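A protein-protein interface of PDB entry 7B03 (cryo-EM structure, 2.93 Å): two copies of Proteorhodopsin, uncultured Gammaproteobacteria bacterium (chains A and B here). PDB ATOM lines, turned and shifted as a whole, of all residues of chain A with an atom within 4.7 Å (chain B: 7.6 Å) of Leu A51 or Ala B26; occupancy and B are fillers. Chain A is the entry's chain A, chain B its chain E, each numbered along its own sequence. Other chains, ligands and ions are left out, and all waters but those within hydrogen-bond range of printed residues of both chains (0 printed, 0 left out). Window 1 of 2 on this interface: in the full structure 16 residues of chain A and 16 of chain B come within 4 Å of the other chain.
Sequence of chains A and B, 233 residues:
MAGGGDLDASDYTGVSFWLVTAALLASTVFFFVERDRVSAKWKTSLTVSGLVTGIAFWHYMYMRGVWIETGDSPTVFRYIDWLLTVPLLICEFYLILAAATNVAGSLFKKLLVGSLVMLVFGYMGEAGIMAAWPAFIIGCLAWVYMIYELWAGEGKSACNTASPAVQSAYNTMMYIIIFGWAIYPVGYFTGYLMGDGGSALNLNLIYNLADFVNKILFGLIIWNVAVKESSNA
OE1 of Glu B34 lies within hydrogen-bond range of OG1 of Thr A47 (3.2 Å).
2 positions are printed for both chains.
Hydrophobic or aromatic side chains of chain B that line the printed part of chain A: Ala B26, Val B29, Phe B30 and Val B33. Printed residues of chain A that touch a printed residue of chain B: Phe A32, Thr A47, Leu A51 and Ile A55. Among the printed residues, 8 pairs touch across the chains. Among the printed residues, no Asp or Glu carboxylate lies within 4 Å of a Lys or Arg side-chain nitrogen of the other chain.
CZ of Phe A32 touches CG1 of Val B29, 3.5 Å away. Phe B30 touches Thr A47. Val B33 touches Thr A47. CD2 of Leu A51 touches O of Ala B26 (3.5 Å). CD1 of Phe B30 touches CD1 of Leu A51 (3.6 Å). Ala B22 touches Ile A55. Ile A55 touches Ala B26 (CD1 to CB, 3.8 Å).
Of the printed residues of chain B, Phe A32 touches Val B29 (3.5 Å). No residue of chain B comes within 4 Å of Gly A50. Printed residues of chain B within 4 Å of Ile A55: Ala B22 (3.6 Å) and Ala B26 (3.8 Å). Leu B25 touches none of the printed residues of chain A. Ala B26 touches just these residues of chain A: Leu A51 and Ile A55. Of the printed residues of chain A, Glu B34 touches Thr A47 (3.2 Å). The nearest printed residue of chain B that does not touch Phe A32 is Val B33 (4.6 Å).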
ATOM      1  N   PHE A  32      19.047  27.569  18.450  1.00  0.00           N
ATOM      2  CA  PHE A  32      18.483  26.454  19.203  1.00  0.00           C
ATOM      3  C   PHE A  32      19.318  26.118  20.430  1.00  0.00           C
ATOM      4  O   PHE A  32      18.784  25.598  21.415  1.00  0.00           O
ATOM      5  CB  PHE A  32      18.330  25.233  18.304  1.00  0.00           C
ATOM      6  CG  PHE A  32      17.118  25.286  17.429  1.00  0.00           C
ATOM      7  CD1 PHE A  32      16.011  26.016  17.811  1.00  0.00           C
ATOM      8  CD2 PHE A  32      17.085  24.615  16.223  1.00  0.00           C
ATOM      9  CE1 PHE A  32      14.898  26.073  17.014  1.00  0.00           C
ATOM     10  CE2 PHE A  32      15.970  24.671  15.421  1.00  0.00           C
ATOM     11  CZ  PHE A  32      14.877  25.401  15.818  1.00  0.00           C
ATOM     12  N   THR A  47      13.261  30.240  19.767  1.00  0.00           N
ATOM     13  CA  THR A  47      12.818  29.089  18.986  1.00  0.00           C
ATOM     14  C   THR A  47      12.291  29.516  17.624  1.00  0.00           C
ATOM     15  O   THR A  47      12.589  28.880  16.610  1.00  0.00           O
ATOM     16  CB  THR A  47      11.742  28.323  19.755  1.00  0.00           C
ATOM     17  OG1 THR A  47      12.225  28.007  21.066  1.00  0.00           O
ATOM     18  CG2 THR A  47      11.383  27.037  19.036  1.00  0.00           C
ATOM     19  N   VAL A  48      11.509  30.592  17.580  1.00  0.00           N
ATOM     20  CA  VAL A  48      10.949  31.037  16.308  1.00  0.00           C
ATOM     21  C   VAL A  48      12.042  31.588  15.400  1.00  0.00           C
ATOM     22  O   VAL A  48      12.021  31.371  14.183  1.00  0.00           O
ATOM     23  CB  VAL A  48       9.822  32.058  16.550  1.00  0.00           C
ATOM     24  CG1 VAL A  48       9.390  32.697  15.246  1.00  0.00           C
ATOM     25  CG2 VAL A  48       8.642  31.373  17.204  1.00  0.00           C
ATOM     26  N   SER A  49      13.024  32.254  16.000  1.00  0.00           N
ATOM     27  CA  SER A  49      14.148  32.791  15.247  1.00  0.00           C
ATOM     28  C   SER A  49      14.877  31.624  14.586  1.00  0.00           C
ATOM     29  O   SER A  49      15.149  31.648  13.386  1.00  0.00           O
ATOM     30  CB  SER A  49      15.097  33.559  16.167  1.00  0.00           C
ATOM     31  OG  SER A  49      14.604  34.860  16.434  1.00  0.00           O
ATOM     32  N   GLY A  50      15.189  30.602  15.380  1.00  0.00           N
ATOM     33  CA  GLY A  50      15.856  29.416  14.876  1.00  0.00           C
ATOM     34  C   GLY A  50      15.044  28.699  13.817  1.00  0.00           C
ATOM     35  O   GLY A  50      15.597  28.165  12.856  1.00  0.00           O
ATOM     36  N   LEU A  51      13.720  28.675  13.979  1.00  0.00           N
ATOM     37  CA  LEU A  51      12.857  28.080  12.965  1.00  0.00           C
ATOM     38  C   LEU A  51      12.952  28.833  11.650  1.00  0.00           C
ATOM     39  O   LEU A  51      12.968  28.221  10.577  1.00  0.00           O
ATOM     40  CB  LEU A  51      11.408  28.056  13.445  1.00  0.00           C
ATOM     41  CG  LEU A  51      11.011  27.005  14.475  1.00  0.00           C
ATOM     42  CD1 LEU A  51       9.523  27.097  14.730  1.00  0.00           C
ATOM     43  CD2 LEU A  51      11.399  25.618  14.005  1.00  0.00           C
ATOM     44  N   VAL A  52      12.988  30.163  11.710  1.00  0.00           N
ATOM     45  CA  VAL A  52      13.108  30.953  10.488  1.00  0.00           C
ATOM     46  C   VAL A  52      14.406  30.618   9.771  1.00  0.00           C
ATOM     47  O   VAL A  52      14.421  30.342   8.564  1.00  0.00           O
ATOM     48  CB  VAL A  52      13.012  32.456  10.804  1.00  0.00           C
ATOM     49  CG1 VAL A  52      13.415  33.276   9.592  1.00  0.00           C
ATOM     50  CG2 VAL A  52      11.611  32.811  11.239  1.00  0.00           C
ATOM     51  N   THR A  53      15.516  30.614  10.512  1.00  0.00           N
ATOM     52  CA  THR A  53      16.796  30.298   9.883  1.00  0.00           C
ATOM     53  C   THR A  53      16.813  28.872   9.341  1.00  0.00           C
ATOM     54  O   THR A  53      17.359  28.619   8.261  1.00  0.00           O
ATOM     55  CB  THR A  53      17.944  30.514  10.866  1.00  0.00           C
ATOM     56  OG1 THR A  53      17.558  30.050  12.164  1.00  0.00           O
ATOM     57  CG2 THR A  53      18.309  31.982  10.938  1.00  0.00           C
ATOM     58  N   GLY A  54      16.218  27.928  10.070  1.00  0.00           N
ATOM     59  CA  GLY A  54      16.205  26.547   9.615  1.00  0.00           C
ATOM     60  C   GLY A  54      15.378  26.337   8.362  1.00  0.00           C
ATOM     61  O   GLY A  54      15.786  25.606   7.457  1.00  0.00           O
ATOM     62  N   ILE A  55      14.201  26.960   8.295  1.00  0.00           N
ATOM     63  CA  ILE A  55      13.384  26.872   7.089  1.00  0.00           C
ATOM     64  C   ILE A  55      14.108  27.510   5.914  1.00  0.00           C
ATOM     65  O   ILE A  55      14.090  26.986   4.791  1.00  0.00           O
ATOM     66  CB  ILE A  55      12.007  27.518   7.329  1.00  0.00           C
ATOM     67  CG1 ILE A  55      11.180  26.662   8.283  1.00  0.00           C
ATOM     68  CG2 ILE A  55      11.258  27.695   6.021  1.00  0.00           C
ATOM     69  CD1 ILE A  55      10.873  25.293   7.741  1.00  0.00           C
ATOM     70  N   LEU A  88       6.489  34.318  10.575  1.00  0.00           N
ATOM     71  CA  LEU A  88       7.201  34.107  11.830  1.00  0.00           C
ATOM     72  C   LEU A  88       8.056  35.314  12.195  1.00  0.00           C
ATOM     73  O   LEU A  88       8.091  35.737  13.359  1.00  0.00           O
ATOM     74  CB  LEU A  88       8.054  32.847  11.739  1.00  0.00           C
ATOM     75  CG  LEU A  88       7.316  31.516  11.611  1.00  0.00           C
ATOM     76  CD1 LEU A  88       8.307  30.371  11.565  1.00  0.00           C
ATOM     77  CD2 LEU A  88       6.339  31.329  12.755  1.00  0.00           C
ATOM     78  N   VAL B  20       3.614  22.093   3.044  1.00  0.00           N
ATOM     79  CA  VAL B  20       3.155  21.307   4.180  1.00  0.00           C
ATOM     80  C   VAL B  20       4.300  20.510   4.784  1.00  0.00           C
ATOM     81  O   VAL B  20       4.401  20.388   6.005  1.00  0.00           O
ATOM     82  CB  VAL B  20       1.989  20.397   3.754  1.00  0.00           C
ATOM     83  CG1 VAL B  20       1.659  19.400   4.848  1.00  0.00           C
ATOM     84  CG2 VAL B  20       0.772  21.237   3.423  1.00  0.00           C
ATOM     85  N   THR B  21       5.177  19.955   3.950  1.00  0.00           N
ATOM     86  CA  THR B  21       6.281  19.160   4.476  1.00  0.00           C
ATOM     87  C   THR B  21       7.227  20.019   5.309  1.00  0.00           C
ATOM     88  O   THR B  21       7.626  19.639   6.421  1.00  0.00           O
ATOM     89  CB  THR B  21       7.023  18.488   3.320  1.00  0.00           C
ATOM     90  OG1 THR B  21       6.094  17.716   2.553  1.00  0.00           O
ATOM     91  CG2 THR B  21       8.105  17.573   3.836  1.00  0.00           C
ATOM     92  N   ALA B  22       7.582  21.196   4.791  1.00  0.00           N
ATOM     93  CA  ALA B  22       8.454  22.088   5.545  1.00  0.00           C
ATOM     94  C   ALA B  22       7.776  22.580   6.817  1.00  0.00           C
ATOM     95  O   ALA B  22       8.414  22.668   7.875  1.00  0.00           O
ATOM     96  CB  ALA B  22       8.883  23.258   4.665  1.00  0.00           C
ATOM     97  N   ALA B  23       6.481  22.896   6.739  1.00  0.00           N
ATOM     98  CA  ALA B  23       5.752  23.325   7.926  1.00  0.00           C
ATOM     99  C   ALA B  23       5.697  22.222   8.972  1.00  0.00           C
ATOM    100  O   ALA B  23       5.809  22.492  10.170  1.00  0.00           O
ATOM    101  CB  ALA B  23       4.344  23.770   7.540  1.00  0.00           C
ATOM    102  N   LEU B  24       5.516  20.973   8.542  1.00  0.00           N
ATOM    103  CA  LEU B  24       5.480  19.858   9.481  1.00  0.00           C
ATOM    104  C   LEU B  24       6.824  19.664  10.164  1.00  0.00           C
ATOM    105  O   LEU B  24       6.879  19.400  11.369  1.00  0.00           O
ATOM    106  CB  LEU B  24       5.058  18.579   8.763  1.00  0.00           C
ATOM    107  CG  LEU B  24       3.591  18.442   8.370  1.00  0.00           C
ATOM    108  CD1 LEU B  24       3.444  17.341   7.346  1.00  0.00           C
ATOM    109  CD2 LEU B  24       2.729  18.160   9.583  1.00  0.00           C
ATOM    110  N   LEU B  25       7.922  19.776   9.411  1.00  0.00           N
ATOM    111  CA  LEU B  25       9.238  19.668  10.040  1.00  0.00           C
ATOM    112  C   LEU B  25       9.459  20.789  11.049  1.00  0.00           C
ATOM    113  O   LEU B  25       9.941  20.553  12.170  1.00  0.00           O
ATOM    114  CB  LEU B  25      10.330  19.679   8.975  1.00  0.00           C
ATOM    115  CG  LEU B  25      11.762  19.467   9.465  1.00  0.00           C
ATOM    116  CD1 LEU B  25      11.921  18.096  10.100  1.00  0.00           C
ATOM    117  CD2 LEU B  25      12.737  19.648   8.322  1.00  0.00           C
ATOM    118  N   ALA B  26       9.070  22.003  10.672  1.00  0.00           N
ATOM    119  CA  ALA B  26       9.207  23.157  11.552  1.00  0.00           C
ATOM    120  C   ALA B  26       8.388  22.961  12.825  1.00  0.00           C
ATOM    121  O   ALA B  26       8.851  23.269  13.924  1.00  0.00           O
ATOM    122  CB  ALA B  26       8.780  24.427  10.833  1.00  0.00           C
ATOM    123  N   SER B  27       7.170  22.447  12.672  1.00  0.00           N
ATOM    124  CA  SER B  27       6.293  22.206  13.811  1.00  0.00           C
ATOM    125  C   SER B  27       6.846  21.118  14.717  1.00  0.00           C
ATOM    126  O   SER B  27       6.738  21.212  15.943  1.00  0.00           O
ATOM    127  CB  SER B  27       4.896  21.832  13.324  1.00  0.00           C
ATOM    128  OG  SER B  27       4.433  22.755  12.362  1.00  0.00           O
ATOM    129  N   THR B  28       7.420  20.066  14.135  1.00  0.00           N
ATOM    130  CA  THR B  28       8.035  19.020  14.942  1.00  0.00           C
ATOM    131  C   THR B  28       9.151  19.592  15.803  1.00  0.00           C
ATOM    132  O   THR B  28       9.221  19.335  17.013  1.00  0.00           O
ATOM    133  CB  THR B  28       8.578  17.916  14.038  1.00  0.00           C
ATOM    134  OG1 THR B  28       7.523  17.419  13.208  1.00  0.00           O
ATOM    135  CG2 THR B  28       9.142  16.780  14.865  1.00  0.00           C
ATOM    136  N   VAL B  29      10.029  20.390  15.189  1.00  0.00           N
ATOM    137  CA  VAL B  29      11.120  20.993  15.948  1.00  0.00           C
ATOM    138  C   VAL B  29      10.571  21.917  17.026  1.00  0.00           C
ATOM    139  O   VAL B  29      11.041  21.911  18.168  1.00  0.00           O
ATOM    140  CB  VAL B  29      12.086  21.729  15.004  1.00  0.00           C
ATOM    141  CG1 VAL B  29      13.224  22.341  15.788  1.00  0.00           C
ATOM    142  CG2 VAL B  29      12.620  20.771  13.959  1.00  0.00           C
ATOM    143  N   PHE B  30       9.557  22.713  16.684  1.00  0.00           N
ATOM    144  CA  PHE B  30       8.976  23.648  17.640  1.00  0.00           C
ATOM    145  C   PHE B  30       8.403  22.918  18.846  1.00  0.00           C
ATOM    146  O   PHE B  30       8.638  23.312  19.993  1.00  0.00           O
ATOM    147  CB  PHE B  30       7.897  24.478  16.946  1.00  0.00           C
ATOM    148  CG  PHE B  30       7.299  25.549  17.808  1.00  0.00           C
ATOM    149  CD1 PHE B  30       7.927  26.772  17.949  1.00  0.00           C
ATOM    150  CD2 PHE B  30       6.102  25.341  18.464  1.00  0.00           C
ATOM    151  CE1 PHE B  30       7.374  27.757  18.737  1.00  0.00           C
ATOM    152  CE2 PHE B  30       5.549  26.325  19.246  1.00  0.00           C
ATOM    153  CZ  PHE B  30       6.185  27.533  19.385  1.00  0.00           C
ATOM    154  N   PHE B  31       7.639  21.854  18.603  1.00  0.00           N
ATOM    155  CA  PHE B  31       7.026  21.114  19.698  1.00  0.00           C
ATOM    156  C   PHE B  31       8.074  20.433  20.566  1.00  0.00           C
ATOM    157  O   PHE B  31       7.956  20.429  21.797  1.00  0.00           O
ATOM    158  CB  PHE B  31       6.037  20.091  19.147  1.00  0.00           C
ATOM    159  CG  PHE B  31       4.826  20.704  18.518  1.00  0.00           C
ATOM    160  CD1 PHE B  31       4.293  21.875  19.017  1.00  0.00           C
ATOM    161  CD2 PHE B  31       4.225  20.116  17.423  1.00  0.00           C
ATOM    162  CE1 PHE B  31       3.185  22.444  18.437  1.00  0.00           C
ATOM    163  CE2 PHE B  31       3.116  20.679  16.842  1.00  0.00           C
ATOM    164  CZ  PHE B  31       2.596  21.843  17.347  1.00  0.00           C
ATOM    165  N   PHE B  32       9.106  19.850  19.954  1.00  0.00           N
ATOM    166  CA  PHE B  32      10.121  19.182  20.760  1.00  0.00           C
ATOM    167  C   PHE B  32      10.978  20.176  21.530  1.00  0.00           C
ATOM    168  O   PHE B  32      11.509  19.838  22.593  1.00  0.00           O
ATOM    169  CB  PHE B  32      10.992  18.290  19.882  1.00  0.00           C
ATOM    170  CG  PHE B  32      10.356  16.976  19.553  1.00  0.00           C
ATOM    171  CD1 PHE B  32       9.416  16.423  20.400  1.00  0.00           C
ATOM    172  CD2 PHE B  32      10.688  16.297  18.398  1.00  0.00           C
ATOM    173  CE1 PHE B  32       8.827  15.222  20.106  1.00  0.00           C
ATOM    174  CE2 PHE B  32      10.097  15.093  18.100  1.00  0.00           C
ATOM    175  CZ  PHE B  32       9.165  14.556  18.954  1.00  0.00           C
ATOM    176  N   VAL B  33      11.115  21.400  21.027  1.00  0.00           N
ATOM    177  CA  VAL B  33      11.960  22.383  21.691  1.00  0.00           C
ATOM    178  C   VAL B  33      11.200  23.105  22.797  1.00  0.00           C
ATOM    179  O   VAL B  33      11.755  23.390  23.863  1.00  0.00           O
ATOM    180  CB  VAL B  33      12.526  23.360  20.645  1.00  0.00           C
ATOM    181  CG1 VAL B  33      13.037  24.612  21.300  1.00  0.00           C
ATOM    182  CG2 VAL B  33      13.640  22.693  19.861  1.00  0.00           C
ATOM    183  N   GLU B  34       9.919  23.385  22.583  1.00  0.00           N
ATOM    184  CA  GLU B  34       9.137  24.192  23.509  1.00  0.00           C
ATOM    185  C   GLU B  34       8.667  23.425  24.736  1.00  0.00           C
ATOM    186  O   GLU B  34       7.874  23.966  25.511  1.00  0.00           O
ATOM    187  CB  GLU B  34       7.931  24.789  22.781  1.00  0.00           C
ATOM    188  CG  GLU B  34       8.261  25.980  21.899  1.00  0.00           C
ATOM    189  CD  GLU B  34       8.662  27.205  22.697  1.00  0.00           C
ATOM    190  OE1 GLU B  34       9.840  27.309  23.091  1.00  0.00           O
ATOM    191  OE2 GLU B  34       7.794  28.064  22.939  1.00  0.00           O
ATOM    192  N   THR B  53       3.369  15.365  14.320  1.00  0.00           N
ATOM    193  CA  THR B  53       3.926  16.145  13.218  1.00  0.00           C
ATOM    194  C   THR B  53       5.120  15.439  12.582  1.00  0.00           C
ATOM    195  O   THR B  53       5.282  15.460  11.357  1.00  0.00           O
ATOM    196  CB  THR B  53       4.319  17.541  13.694  1.00  0.00           C
ATOM    197  OG1 THR B  53       4.918  17.455  14.992  1.00  0.00           O
ATOM    198  CG2 THR B  53       3.103  18.441  13.755  1.00  0.00           C
ATOM    199  N   PHE B  57       5.475  14.212   8.742  1.00  0.00           N
ATOM    200  CA  PHE B  57       6.571  14.645   7.878  1.00  0.00           C
ATOM    201  C   PHE B  57       7.302  13.452   7.270  1.00  0.00           C
ATOM    202  O   PHE B  57       7.625  13.449   6.074  1.00  0.00           O
ATOM    203  CB  PHE B  57       7.529  15.526   8.683  1.00  0.00           C
ATOM    204  CG  PHE B  57       8.877  15.704   8.052  1.00  0.00           C
ATOM    205  CD1 PHE B  57       9.066  16.619   7.036  1.00  0.00           C
ATOM    206  CD2 PHE B  57       9.963  14.972   8.494  1.00  0.00           C
ATOM    207  CE1 PHE B  57      10.306  16.789   6.460  1.00  0.00           C
ATOM    208  CE2 PHE B  57      11.203  15.138   7.921  1.00  0.00           C
ATOM    209  CZ  PHE B  57      11.375  16.047   6.904  1.00  0.00           C
ATOM    210  N   ILE B 216      -1.013  20.920  12.802  1.00  0.00           N
ATOM    211  CA  ILE B 216      -0.220  22.035  13.295  1.00  0.00           C
ATOM    212  C   ILE B 216      -1.037  22.923  14.219  1.00  0.00           C
ATOM    213  O   ILE B 216      -0.593  23.264  15.316  1.00  0.00           O
ATOM    214  CB  ILE B 216       0.366  22.821  12.103  1.00  0.00           C
ATOM    215  CG1 ILE B 216       1.205  21.882  11.237  1.00  0.00           C
ATOM    216  CG2 ILE B 216       1.220  23.972  12.587  1.00  0.00           C
ATOM    217  CD1 ILE B 216       1.811  22.535  10.030  1.00  0.00           C
